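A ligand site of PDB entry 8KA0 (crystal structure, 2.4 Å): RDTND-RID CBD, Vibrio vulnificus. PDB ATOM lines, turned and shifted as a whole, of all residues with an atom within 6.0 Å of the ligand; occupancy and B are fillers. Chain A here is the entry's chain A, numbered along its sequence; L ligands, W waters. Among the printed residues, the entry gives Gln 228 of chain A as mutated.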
ATOM      1  N   GLY A  42      -6.155  12.005  22.777  1.00  0.00           N
ATOM      2  CA  GLY A  42      -6.617  10.924  21.913  1.00  0.00           C
ATOM      3  C   GLY A  42      -7.411   9.862  22.668  1.00  0.00           C
ATOM      4  O   GLY A  42      -7.756   8.827  22.126  1.00  0.00           O
ATOM      5  N   PHE A  43      -7.698  10.112  23.943  1.00  0.00           N
ATOM      6  CA  PHE A  43      -8.394   9.157  24.791  1.00  0.00           C
ATOM      7  C   PHE A  43      -9.520   9.872  25.588  1.00  0.00           C
ATOM      8  O   PHE A  43      -9.471   9.935  26.829  1.00  0.00           O
ATOM      9  CB  PHE A  43      -7.377   8.421  25.672  1.00  0.00           C
ATOM     10  CG  PHE A  43      -6.576   7.428  24.902  1.00  0.00           C
ATOM     11  CD1 PHE A  43      -5.260   7.700  24.561  1.00  0.00           C
ATOM     12  CD2 PHE A  43      -7.169   6.285  24.391  1.00  0.00           C
ATOM     13  CE1 PHE A  43      -4.536   6.838  23.760  1.00  0.00           C
ATOM     14  CE2 PHE A  43      -6.455   5.418  23.581  1.00  0.00           C
ATOM     15  CZ  PHE A  43      -5.126   5.695  23.279  1.00  0.00           C
ATOM     16  N   SER A 122      13.459   3.770  24.953  1.00  0.00           N
ATOM     17  CA  SER A 122      13.073   3.468  23.569  1.00  0.00           C
ATOM     18  C   SER A 122      11.612   3.068  23.540  1.00  0.00           C
ATOM     19  O   SER A 122      10.988   2.865  24.601  1.00  0.00           O
ATOM     20  CB  SER A 122      13.939   2.372  23.003  1.00  0.00           C
ATOM     21  OG  SER A 122      15.280   2.794  22.872  1.00  0.00           O
ATOM     22  N   PHE A 123      11.062   2.997  22.325  1.00  0.00           N
ATOM     23  CA  PHE A 123       9.621   2.898  22.107  1.00  0.00           C
ATOM     24  C   PHE A 123       9.367   1.918  20.975  1.00  0.00           C
ATOM     25  O   PHE A 123      10.228   1.699  20.148  1.00  0.00           O
ATOM     26  CB  PHE A 123       9.061   4.293  21.785  1.00  0.00           C
ATOM     27  CG  PHE A 123       9.415   5.325  22.808  1.00  0.00           C
ATOM     28  CD1 PHE A 123      10.657   5.937  22.789  1.00  0.00           C
ATOM     29  CD2 PHE A 123       8.522   5.664  23.810  1.00  0.00           C
ATOM     30  CE1 PHE A 123      10.996   6.884  23.743  1.00  0.00           C
ATOM     31  CE2 PHE A 123       8.860   6.611  24.753  1.00  0.00           C
ATOM     32  CZ  PHE A 123      10.091   7.205  24.746  1.00  0.00           C
ATOM     33  N   TRP A 124       8.166   1.366  20.940  1.00  0.00           N
ATOM     34  CA  TRP A 124       7.792   0.355  19.959  1.00  0.00           C
ATOM     35  C   TRP A 124       6.353   0.596  19.473  1.00  0.00           C
ATOM     36  O   TRP A 124       5.559   1.205  20.188  1.00  0.00           O
ATOM     37  CB  TRP A 124       7.943  -1.049  20.571  1.00  0.00           C
ATOM     38  CG  TRP A 124       7.305  -1.222  21.924  1.00  0.00           C
ATOM     39  CD1 TRP A 124       7.863  -0.962  23.141  1.00  0.00           C
ATOM     40  CD2 TRP A 124       6.006  -1.778  22.190  1.00  0.00           C
ATOM     41  NE1 TRP A 124       6.982  -1.249  24.144  1.00  0.00           N
ATOM     42  CE2 TRP A 124       5.849  -1.774  23.601  1.00  0.00           C
ATOM     43  CE3 TRP A 124       4.966  -2.281  21.398  1.00  0.00           C
ATOM     44  CZ2 TRP A 124       4.676  -2.236  24.208  1.00  0.00           C
ATOM     45  CZ3 TRP A 124       3.825  -2.760  22.011  1.00  0.00           C
ATOM     46  CH2 TRP A 124       3.687  -2.732  23.400  1.00  0.00           C
ATOM     47  N   SER A 125       6.086   0.168  18.238  1.00  0.00           N
ATOM     48  CA  SER A 125       4.729  -0.155  17.768  1.00  0.00           C
ATOM     49  C   SER A 125       4.831  -1.448  16.950  1.00  0.00           C
ATOM     50  O   SER A 125       5.806  -1.609  16.214  1.00  0.00           O
ATOM     51  CB  SER A 125       4.124   0.974  16.914  1.00  0.00           C
ATOM     52  OG  SER A 125       3.956   2.189  17.647  1.00  0.00           O
ATOM     53  N   GLY A 126       3.806  -2.347  17.066  1.00  0.00           N
ATOM     54  CA  GLY A 126       3.825  -3.651  16.406  1.00  0.00           C
ATOM     55  C   GLY A 126       4.490  -4.746  17.255  1.00  0.00           C
ATOM     56  O   GLY A 126       5.030  -4.439  18.313  1.00  0.00           O
ATOM     57  N   LYS A 127       4.519  -5.985  16.745  1.00  0.00           N
ATOM     58  CA  LYS A 127       4.731  -7.206  17.535  1.00  0.00           C
ATOM     59  C   LYS A 127       6.183  -7.715  17.473  1.00  0.00           C
ATOM     60  O   LYS A 127       6.555  -8.568  18.262  1.00  0.00           O
ATOM     61  CB  LYS A 127       3.792  -8.326  17.037  1.00  0.00           C
ATOM     62  CG  LYS A 127       2.390  -7.897  16.631  1.00  0.00           C
ATOM     63  CD  LYS A 127       1.353  -9.035  16.614  1.00  0.00           C
ATOM     64  CE  LYS A 127       0.370  -8.999  17.771  1.00  0.00           C
ATOM     65  NZ  LYS A 127       1.042  -8.842  19.086  1.00  0.00           N
ATOM     66  N   ASP A 149       9.234  -0.038  27.985  1.00  0.00           N
ATOM     67  CA  ASP A 149       8.455   0.156  29.195  1.00  0.00           C
ATOM     68  C   ASP A 149       8.114  -1.216  29.814  1.00  0.00           C
ATOM     69  O   ASP A 149       7.925  -1.287  31.026  1.00  0.00           O
ATOM     70  CB  ASP A 149       7.241   1.049  28.958  1.00  0.00           C
ATOM     71  CG  ASP A 149       6.271   0.568  27.918  1.00  0.00           C
ATOM     72  OD1 ASP A 149       6.579  -0.391  27.275  1.00  0.00           O
ATOM     73  OD2 ASP A 149       5.215   1.236  27.733  1.00  0.00           O
ATOM     74  N   ILE A 150       8.084  -2.261  28.971  1.00  0.00           N
ATOM     75  CA  ILE A 150       7.825  -3.643  29.391  1.00  0.00           C
ATOM     76  C   ILE A 150       8.930  -4.138  30.346  1.00  0.00           C
ATOM     77  O   ILE A 150       8.738  -5.132  31.035  1.00  0.00           O
ATOM     78  CB  ILE A 150       7.701  -4.602  28.176  1.00  0.00           C
ATOM     79  CG1 ILE A 150       8.985  -4.650  27.352  1.00  0.00           C
ATOM     80  CG2 ILE A 150       6.501  -4.225  27.338  1.00  0.00           C
ATOM     81  CD1 ILE A 150       9.226  -5.965  26.651  1.00  0.00           C
ATOM     82  N   ILE A 159      -0.010  -2.057  34.341  1.00  0.00           N
ATOM     83  CA  ILE A 159      -0.605  -2.556  33.115  1.00  0.00           C
ATOM     84  C   ILE A 159      -1.262  -3.912  33.382  1.00  0.00           C
ATOM     85  O   ILE A 159      -2.244  -4.254  32.736  1.00  0.00           O
ATOM     86  CB  ILE A 159       0.441  -2.581  31.972  1.00  0.00           C
ATOM     87  CG1 ILE A 159       0.661  -1.167  31.436  1.00  0.00           C
ATOM     88  CG2 ILE A 159       0.055  -3.568  30.872  1.00  0.00           C
ATOM     89  CD1 ILE A 159       1.712  -1.067  30.365  1.00  0.00           C
ATOM     90  N   LYS A 163      -5.363  -4.725  32.822  1.00  0.00           N
ATOM     91  CA  LYS A 163      -5.888  -5.795  31.974  1.00  0.00           C
ATOM     92  C   LYS A 163      -6.986  -6.569  32.721  1.00  0.00           C
ATOM     93  O   LYS A 163      -7.964  -7.013  32.104  1.00  0.00           O
ATOM     94  CB  LYS A 163      -4.766  -6.718  31.507  1.00  0.00           C
ATOM     95  CG  LYS A 163      -3.953  -6.216  30.332  1.00  0.00           C
ATOM     96  CD  LYS A 163      -2.598  -6.890  30.187  1.00  0.00           C
ATOM     97  CE  LYS A 163      -1.958  -6.659  28.834  1.00  0.00           C
ATOM     98  NZ  LYS A 163      -0.586  -7.235  28.749  1.00  0.00           N
ATOM     99  N   PHE A 192      -8.088   2.425  28.701  1.00  0.00           N
ATOM    100  CA  PHE A 192      -7.175   2.916  27.677  1.00  0.00           C
ATOM    101  C   PHE A 192      -6.513   4.215  28.153  1.00  0.00           C
ATOM    102  O   PHE A 192      -5.343   4.469  27.876  1.00  0.00           O
ATOM    103  CB  PHE A 192      -7.885   3.187  26.341  1.00  0.00           C
ATOM    104  CG  PHE A 192      -8.505   2.006  25.662  1.00  0.00           C
ATOM    105  CD1 PHE A 192      -7.945   0.739  25.765  1.00  0.00           C
ATOM    106  CD2 PHE A 192      -9.635   2.165  24.865  1.00  0.00           C
ATOM    107  CE1 PHE A 192      -8.540  -0.353  25.155  1.00  0.00           C
ATOM    108  CE2 PHE A 192     -10.231   1.073  24.255  1.00  0.00           C
ATOM    109  CZ  PHE A 192      -9.681  -0.190  24.400  1.00  0.00           C
ATOM    110  N   THR A 195      -3.520   3.474  30.214  1.00  0.00           N
ATOM    111  CA  THR A 195      -2.360   3.006  29.447  1.00  0.00           C
ATOM    112  C   THR A 195      -1.669   4.209  28.824  1.00  0.00           C
ATOM    113  O   THR A 195      -0.445   4.291  28.831  1.00  0.00           O
ATOM    114  CB  THR A 195      -2.761   1.972  28.398  1.00  0.00           C
ATOM    115  OG1 THR A 195      -3.360   0.855  29.044  1.00  0.00           O
ATOM    116  CG2 THR A 195      -1.610   1.469  27.571  1.00  0.00           C
ATOM    117  N   SER A 199       2.032   5.545  29.699  1.00  0.00           N
ATOM    118  CA  SER A 199       2.914   5.625  28.533  1.00  0.00           C
ATOM    119  C   SER A 199       3.661   6.945  28.539  1.00  0.00           C
ATOM    120  O   SER A 199       4.872   6.963  28.365  1.00  0.00           O
ATOM    121  CB  SER A 199       2.163   5.432  27.265  1.00  0.00           C
ATOM    122  OG  SER A 199       1.761   4.081  27.186  1.00  0.00           O
ATOM    123  N   TYR A 202       6.337   7.094  31.333  1.00  0.00           N
ATOM    124  CA  TYR A 202       7.534   6.422  30.852  1.00  0.00           C
ATOM    125  C   TYR A 202       8.300   7.342  29.897  1.00  0.00           C
ATOM    126  O   TYR A 202       9.483   7.630  30.121  1.00  0.00           O
ATOM    127  CB  TYR A 202       7.147   5.082  30.209  1.00  0.00           C
ATOM    128  CG  TYR A 202       8.276   4.410  29.473  1.00  0.00           C
ATOM    129  CD1 TYR A 202       9.255   3.711  30.157  1.00  0.00           C
ATOM    130  CD2 TYR A 202       8.394   4.520  28.097  1.00  0.00           C
ATOM    131  CE1 TYR A 202      10.325   3.130  29.477  1.00  0.00           C
ATOM    132  CE2 TYR A 202       9.442   3.937  27.420  1.00  0.00           C
ATOM    133  CZ  TYR A 202      10.416   3.247  28.104  1.00  0.00           C
ATOM    134  OH  TYR A 202      11.432   2.658  27.419  1.00  0.00           O
ATOM    135  N   ARG A 219       2.767   4.918  12.748  1.00  0.00           N
ATOM    136  CA  ARG A 219       1.345   4.620  12.908  1.00  0.00           C
ATOM    137  C   ARG A 219       0.663   5.864  13.509  1.00  0.00           C
ATOM    138  O   ARG A 219       1.205   6.469  14.419  1.00  0.00           O
ATOM    139  CB  ARG A 219       1.142   3.346  13.746  1.00  0.00           C
ATOM    140  CG  ARG A 219       1.565   2.054  13.048  1.00  0.00           C
ATOM    141  CD  ARG A 219       2.876   1.474  13.551  1.00  0.00           C
ATOM    142  NE  ARG A 219       3.108   0.078  13.152  1.00  0.00           N
ATOM    143  CZ  ARG A 219       2.581  -0.986  13.771  1.00  0.00           C
ATOM    144  NH1 ARG A 219       1.789  -0.835  14.831  1.00  0.00           N
ATOM    145  NH2 ARG A 219       2.843  -2.201  13.321  1.00  0.00           N
ATOM    146  N   GLY A 221      -2.727   7.450  15.371  1.00  0.00           N
ATOM    147  CA  GLY A 221      -3.893   7.106  16.180  1.00  0.00           C
ATOM    148  C   GLY A 221      -3.612   6.099  17.297  1.00  0.00           C
ATOM    149  O   GLY A 221      -4.534   5.672  17.970  1.00  0.00           O
ATOM    150  N   ASN A 222      -2.336   5.715  17.494  1.00  0.00           N
ATOM    151  CA  ASN A 222      -1.959   4.724  18.502  1.00  0.00           C
ATOM    152  C   ASN A 222      -1.234   5.428  19.658  1.00  0.00           C
ATOM    153  O   ASN A 222      -1.135   6.656  19.693  1.00  0.00           O
ATOM    154  CB  ASN A 222      -1.175   3.562  17.892  1.00  0.00           C
ATOM    155  CG  ASN A 222       0.293   3.823  17.628  1.00  0.00           C
ATOM    156  OD1 ASN A 222       0.783   4.944  17.746  1.00  0.00           O
ATOM    157  ND2 ASN A 222       0.996   2.788  17.178  1.00  0.00           N
ATOM    158  N   TYR A 223      -0.735   4.623  20.626  1.00  0.00           N
ATOM    159  CA  TYR A 223      -0.251   5.161  21.893  1.00  0.00           C
ATOM    160  C   TYR A 223       0.958   6.035  21.619  1.00  0.00           C
ATOM    161  O   TYR A 223       1.001   7.159  22.060  1.00  0.00           O
ATOM    162  CB  TYR A 223      -0.002   4.051  22.911  1.00  0.00           C
ATOM    163  CG  TYR A 223      -1.268   3.542  23.606  1.00  0.00           C
ATOM    164  CD1 TYR A 223      -1.749   2.285  23.355  1.00  0.00           C
ATOM    165  CD2 TYR A 223      -1.927   4.316  24.561  1.00  0.00           C
ATOM    166  CE1 TYR A 223      -2.867   1.794  24.006  1.00  0.00           C
ATOM    167  CE2 TYR A 223      -3.052   3.856  25.213  1.00  0.00           C
ATOM    168  CZ  TYR A 223      -3.531   2.590  24.932  1.00  0.00           C
ATOM    169  OH  TYR A 223      -4.644   2.126  25.553  1.00  0.00           O
ATOM    170  N   PHE A 224       1.911   5.543  20.841  1.00  0.00           N
ATOM    171  CA  PHE A 224       3.099   6.328  20.528  1.00  0.00           C
ATOM    172  C   PHE A 224       2.691   7.700  19.950  1.00  0.00           C
ATOM    173  O   PHE A 224       3.204   8.702  20.345  1.00  0.00           O
ATOM    174  CB  PHE A 224       3.994   5.636  19.502  1.00  0.00           C
ATOM    175  CG  PHE A 224       5.244   6.418  19.224  1.00  0.00           C
ATOM    176  CD1 PHE A 224       6.202   6.573  20.231  1.00  0.00           C
ATOM    177  CD2 PHE A 224       5.444   7.058  18.027  1.00  0.00           C
ATOM    178  CE1 PHE A 224       7.332   7.353  20.024  1.00  0.00           C
ATOM    179  CE2 PHE A 224       6.547   7.868  17.833  1.00  0.00           C
ATOM    180  CZ  PHE A 224       7.490   8.026  18.831  1.00  0.00           C
ATOM    181  N   TRP A 225       1.822   7.698  18.966  1.00  0.00           N
ATOM    182  CA  TRP A 225       1.388   8.922  18.308  1.00  0.00           C
ATOM    183  C   TRP A 225       0.675   9.835  19.300  1.00  0.00           C
ATOM    184  O   TRP A 225       0.907  11.039  19.262  1.00  0.00           O
ATOM    185  CB  TRP A 225       0.472   8.584  17.114  1.00  0.00           C
ATOM    186  CG  TRP A 225      -0.021   9.810  16.442  1.00  0.00           C
ATOM    187  CD1 TRP A 225      -1.235  10.424  16.613  1.00  0.00           C
ATOM    188  CD2 TRP A 225       0.718  10.621  15.528  1.00  0.00           C
ATOM    189  NE1 TRP A 225      -1.292  11.558  15.838  1.00  0.00           N
ATOM    190  CE2 TRP A 225      -0.117  11.703  15.167  1.00  0.00           C
ATOM    191  CE3 TRP A 225       1.997  10.542  14.966  1.00  0.00           C
ATOM    192  CZ2 TRP A 225       0.286  12.680  14.267  1.00  0.00           C
ATOM    193  CZ3 TRP A 225       2.402  11.540  14.106  1.00  0.00           C
ATOM    194  CH2 TRP A 225       1.567  12.586  13.764  1.00  0.00           C
ATOM    195  N   ASN A 226      -0.233   9.267  20.131  1.00  0.00           N
ATOM    196  CA  ASN A 226      -1.150  10.029  20.969  1.00  0.00           C
ATOM    197  C   ASN A 226      -0.412  10.657  22.173  1.00  0.00           C
ATOM    198  O   ASN A 226      -0.600  11.856  22.446  1.00  0.00           O
ATOM    199  CB  ASN A 226      -2.355   9.192  21.414  1.00  0.00           C
ATOM    200  CG  ASN A 226      -3.368   8.977  20.311  1.00  0.00           C
ATOM    201  OD1 ASN A 226      -3.246   9.575  19.262  1.00  0.00           O
ATOM    202  ND2 ASN A 226      -4.348   8.142  20.543  1.00  0.00           N
ATOM    203  N   VAL A 227       0.396   9.859  22.892  1.00  0.00           N
ATOM    204  CA  VAL A 227       0.776  10.192  24.276  1.00  0.00           C
ATOM    205  C   VAL A 227       2.320  10.189  24.473  1.00  0.00           C
ATOM    206  O   VAL A 227       2.809  10.773  25.439  1.00  0.00           O
ATOM    207  CB  VAL A 227       0.078   9.283  25.285  1.00  0.00           C
ATOM    208  CG1 VAL A 227      -1.418   9.406  25.226  1.00  0.00           C
ATOM    209  CG2 VAL A 227       0.488   7.856  25.130  1.00  0.00           C
ATOM    210  N   GLN A 228       3.089   9.555  23.570  1.00  0.00           N
ATOM    211  CA  GLN A 228       4.531   9.391  23.795  1.00  0.00           C
ATOM    212  C   GLN A 228       5.308  10.413  22.981  1.00  0.00           C
ATOM    213  O   GLN A 228       6.187  11.081  23.539  1.00  0.00           O
ATOM    214  CB  GLN A 228       4.991   7.977  23.514  1.00  0.00           C
ATOM    215  CG  GLN A 228       4.476   7.019  24.576  1.00  0.00           C
ATOM    216  CD  GLN A 228       4.995   5.620  24.400  1.00  0.00           C
ATOM    217  OE1 GLN A 228       5.177   5.129  23.263  1.00  0.00           O
ATOM    218  NE2 GLN A 228       5.227   4.964  25.546  1.00  0.00           N
ATOM    219  N   ARG A 276      -4.433   3.045  11.954  1.00  0.00           N
ATOM    220  CA  ARG A 276      -5.524   2.192  12.397  1.00  0.00           C
ATOM    221  C   ARG A 276      -6.741   2.536  11.551  1.00  0.00           C
ATOM    222  O   ARG A 276      -6.930   3.705  11.221  1.00  0.00           O
ATOM    223  CB  ARG A 276      -5.873   2.440  13.869  1.00  0.00           C
ATOM    224  CG  ARG A 276      -4.701   2.396  14.834  1.00  0.00           C
ATOM    225  CD  ARG A 276      -5.190   2.440  16.286  1.00  0.00           C
ATOM    226  NE  ARG A 276      -5.079   1.128  16.903  1.00  0.00           N
ATOM    227  CZ  ARG A 276      -5.938   0.598  17.751  1.00  0.00           C
ATOM    228  NH1 ARG A 276      -7.039   1.242  18.093  1.00  0.00           N
ATOM    229  NH2 ARG A 276      -5.654  -0.565  18.293  1.00  0.00           N
ATOM    230  N   ASP A 278      -9.710   2.675  12.604  1.00  0.00           N
ATOM    231  CA  ASP A 278     -10.611   3.469  13.441  1.00  0.00           C
ATOM    232  C   ASP A 278     -10.086   4.918  13.600  1.00  0.00           C
ATOM    233  O   ASP A 278     -10.599   5.679  14.430  1.00  0.00           O
ATOM    234  CB  ASP A 278     -10.821   2.812  14.809  1.00  0.00           C
ATOM    235  CG  ASP A 278      -9.605   2.785  15.729  1.00  0.00           C
ATOM    236  OD1 ASP A 278      -9.758   2.323  16.913  1.00  0.00           O
ATOM    237  OD2 ASP A 278      -8.512   3.191  15.290  1.00  0.00           O
ATOM    238  N   ASP A 299      -8.075  -2.252  14.824  1.00  0.00           N
ATOM    239  CA  ASP A 299      -6.636  -2.102  14.952  1.00  0.00           C
ATOM    240  C   ASP A 299      -5.930  -2.446  13.637  1.00  0.00           C
ATOM    241  O   ASP A 299      -4.705  -2.380  13.553  1.00  0.00           O
ATOM    242  CB  ASP A 299      -6.074  -2.973  16.085  1.00  0.00           C
ATOM    243  CG  ASP A 299      -6.512  -4.424  15.998  1.00  0.00           C
ATOM    244  OD1 ASP A 299      -7.413  -4.709  15.185  1.00  0.00           O
ATOM    245  OD2 ASP A 299      -5.933  -5.261  16.748  1.00  0.00           O
ATOM    246  N   LEU A 301      -4.050  -2.205  10.540  1.00  0.00           N
ATOM    247  CA  LEU A 301      -3.161  -1.143  10.078  1.00  0.00           C
ATOM    248  C   LEU A 301      -3.249  -1.037   8.561  1.00  0.00           C
ATOM    249  O   LEU A 301      -2.903  -1.992   7.854  1.00  0.00           O
ATOM    250  CB  LEU A 301      -1.719  -1.459  10.502  1.00  0.00           C
ATOM    251  CG  LEU A 301      -1.465  -1.573  12.003  1.00  0.00           C
ATOM    252  CD1 LEU A 301      -0.011  -1.895  12.265  1.00  0.00           C
ATOM    253  CD2 LEU A 301      -1.876  -0.299  12.730  1.00  0.00           C
HETATM  254  P1  LIG L   1       0.874  -0.603  18.717  1.00  0.00           P
HETATM  255  O1  LIG L   1       0.331   0.042  17.509  1.00  0.00           O
HETATM  256  O2  LIG L   1       1.719  -1.841  18.563  1.00  0.00           O
HETATM  257  O3  LIG L   1      -0.310  -0.925  19.728  1.00  0.00           O
HETATM  258  C1  LIG L   1       0.013  -1.738  20.893  1.00  0.00           C
HETATM  259  C2  LIG L   1      -1.243  -2.028  21.680  1.00  0.00           C
HETATM  260  O4  LIG L   1      -1.971  -0.784  21.883  1.00  0.00           O
HETATM  261  C3  LIG L   1      -2.240  -2.974  20.999  1.00  0.00           C
HETATM  262  O5  LIG L   1      -2.919  -3.823  21.947  1.00  0.00           O
HETATM  263  C4  LIG L   1      -3.238  -1.990  20.371  1.00  0.00           C
HETATM  264  O6  LIG L   1      -4.511  -2.560  20.172  1.00  0.00           O
HETATM  265  C5  LIG L   1      -3.286  -0.913  21.443  1.00  0.00           C
HETATM  266  N1  LIG L   1      -3.745   0.379  20.948  1.00  0.00           N
HETATM  267  C6  LIG L   1      -3.132   1.166  20.016  1.00  0.00           C
HETATM  268  N2  LIG L   1      -3.769   2.260  19.757  1.00  0.00           N
HETATM  269  C7  LIG L   1      -4.901   2.201  20.556  1.00  0.00           C
HETATM  270  C8  LIG L   1      -5.981   3.086  20.727  1.00  0.00           C
HETATM  271  N3  LIG L   1      -6.087   4.242  20.078  1.00  0.00           N
HETATM  272  N4  LIG L   1      -6.950   2.733  21.617  1.00  0.00           N
HETATM  273  C9  LIG L   1      -6.812   1.583  22.284  1.00  0.00           C
HETATM  274  N5  LIG L   1      -5.843   0.663  22.203  1.00  0.00           N
HETATM  275  C10 LIG L   1      -4.913   1.041  21.296  1.00  0.00           C
HETATM  276  O7  LIG L   1       1.715   0.490  19.504  1.00  0.00           O
HETATM  277  P2  LIG L   1       1.274   1.679  20.393  1.00  0.00           P
HETATM  278  O8  LIG L   1      -0.227   1.847  20.305  1.00  0.00           O
HETATM  279  O9  LIG L   1       2.178   2.812  20.031  1.00  0.00           O
HETATM  280  O10 LIG L   1       1.644   1.150  21.839  1.00  0.00           O
HETATM  281  C11 LIG L   1       3.034   0.839  22.087  1.00  0.00           C
HETATM  282  C12 LIG L   1       3.780   2.056  22.604  1.00  0.00           C
HETATM  283  O11 LIG L   1       3.066   2.700  23.673  1.00  0.00           O
HETATM  284  C13 LIG L   1       5.164   1.766  23.194  1.00  0.00           C
HETATM  285  O12 LIG L   1       6.091   2.791  22.929  1.00  0.00           O
HETATM  286  C14 LIG L   1       4.917   1.642  24.723  1.00  0.00           C
HETATM  287  O13 LIG L   1       5.809   2.442  25.492  1.00  0.00           O
HETATM  288  C15 LIG L   1       3.465   2.131  24.915  1.00  0.00           C
HETATM  289  N6  LIG L   1       2.520   1.017  25.321  1.00  0.00           N
HETATM  290  C16 LIG L   1       2.978  -0.006  26.120  1.00  0.00           C
HETATM  291  C17 LIG L   1       2.129  -1.052  26.489  1.00  0.00           C
HETATM  292  C18 LIG L   1       2.674  -2.157  27.349  1.00  0.00           C
HETATM  293  O14 LIG L   1       1.972  -3.165  27.533  1.00  0.00           O
HETATM  294  N7  LIG L   1       3.885  -1.990  27.900  1.00  0.00           N
HETATM  295  C19 LIG L   1       0.801  -1.030  26.101  1.00  0.00           C
HETATM  296  C20 LIG L   1       0.342   0.016  25.312  1.00  0.00           C
HETATM  297  C21 LIG L   1       1.206   1.035  24.942  1.00  0.00           C
HETATM  298  O   HOH W   1       8.883   1.365  25.463  1.00  0.00           O
HETATM  299  O   HOH W   2      -9.329   3.930  21.261  1.00  0.00           O
HETATM  300  O   HOH W   3      -5.143  -0.726  25.245  1.00  0.00           O
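The side-chain amide oxygen (OD1) of Asn 222 sits at hydrogen-bond distance from the backbone NH (N) of Phe 224.
ND2 of Asn 222 is in hydrogen-bond range of OG of Ser 125 (3.1 Å).
The side-chain hydroxyl (OG) of Ser 199 lies within hydrogen-bond range of the backbone carbonyl oxygen (O) of Thr 195, at 2.8 Å.
OD1 of Asp 149 is in hydrogen-bond range of NE1 of Trp 124 (3.3 Å).
The backbone NH of Trp 225 lies within hydrogen-bond range of the side-chain amide oxygen of Asn 222.
The side-chain amide nitrogen of Gln 228 is in hydrogen-bond range of the backbone carbonyl oxygen of Ser 199 (3.5 Å).
The side-chain hydroxyl (OH) of Tyr 223 is in hydrogen-bond range of the backbone carbonyl oxygen (O) of Phe 192.
NH1 of Arg 276 is in salt-bridge range of OD1 of Asp 278.
CE2 of Phe 43 touches N4 of the ligand, 3.4 Å away.
Phe 123 touches the ligand (CB to O12, 3.5 Å).
Ile 150 touches the ligand.
Ile 159 touches the ligand.
Phe 192 touches the ligand (CD1 to C9, 3.8 Å).
CG2 of Thr 195 touches C20 of the ligand, 3.3 Å away.
Ser 199 touches the ligand (OG to C15, 3.4 Å).
Hydrophobic or aromatic side chains within 4 Å of the ligand: Phe 43, Phe 123, Trp 124, Ile 150, Ile 159, Phe 192, Tyr 223 and Phe 224.
18 residues have an atom within 4 Å of the ligand: Phe 43, Phe 123, Trp 124, Ser 125, Gly 126, Asp 149, Ile 150, Ile 159, Phe 192, Thr 195, Ser 199, Arg 219, Gly 221, Asn 222, Tyr 223, Phe 224, Gln 228 and Arg 276.
The nearest printed residue that does not touch the ligand is Tyr 202 (4.2 Å).
Water W1 lies within hydrogen-bond range of O of Ser 122, N of Asp 149, O13 of the ligand, OH of Tyr 202 and NE1 of Trp 124.
Water W3 bridges the side-chain hydroxyl of Tyr 223 (2.9 Å) and a nitrogen (N5) of the ligand (3.4 Å).
The guanidinium group of Arg 219 is in salt-bridge range of an oxygen (O1) of the ligand (3.2 Å).
N3 of the ligand lies within hydrogen-bond range of O of Gly 221.
The backbone carbonyl oxygen (O) of Trp 124 lies close to an oxygen (O12) of the ligand (3.2 Å).
O6 of the ligand sits at hydrogen-bond distance from NH2 of Arg 276, at 3.0 Å.
The side-chain amide nitrogen (ND2) of Asn 222 is in hydrogen-bond range of an oxygen (O1) of the ligand (2.8 Å).
N of Tyr 223 is in hydrogen-bond range of O8 of the ligand, 2.8 Å away.
The side-chain hydroxyl (OG) of Ser 125 is in hydrogen-bond range of an oxygen (O9) of the ligand, 3.0 Å away.
O12 of the ligand is in hydrogen-bond range of OE1 of Gln 228 (2.5 Å).
N of Gly 126 is in hydrogen-bond range of O2 of the ligand, at 2.6 Å.
The backbone NH of Phe 224 lies within hydrogen-bond range of an oxygen (O9) of the ligand (2.9 Å).
The side-chain carboxylate of Asp 149 lies within hydrogen-bond range of an oxygen (O13) of the ligand.
The backbone NH (N) of Trp 124 is in hydrogen-bond range of an oxygen (O12) of the ligand (3.2 Å).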
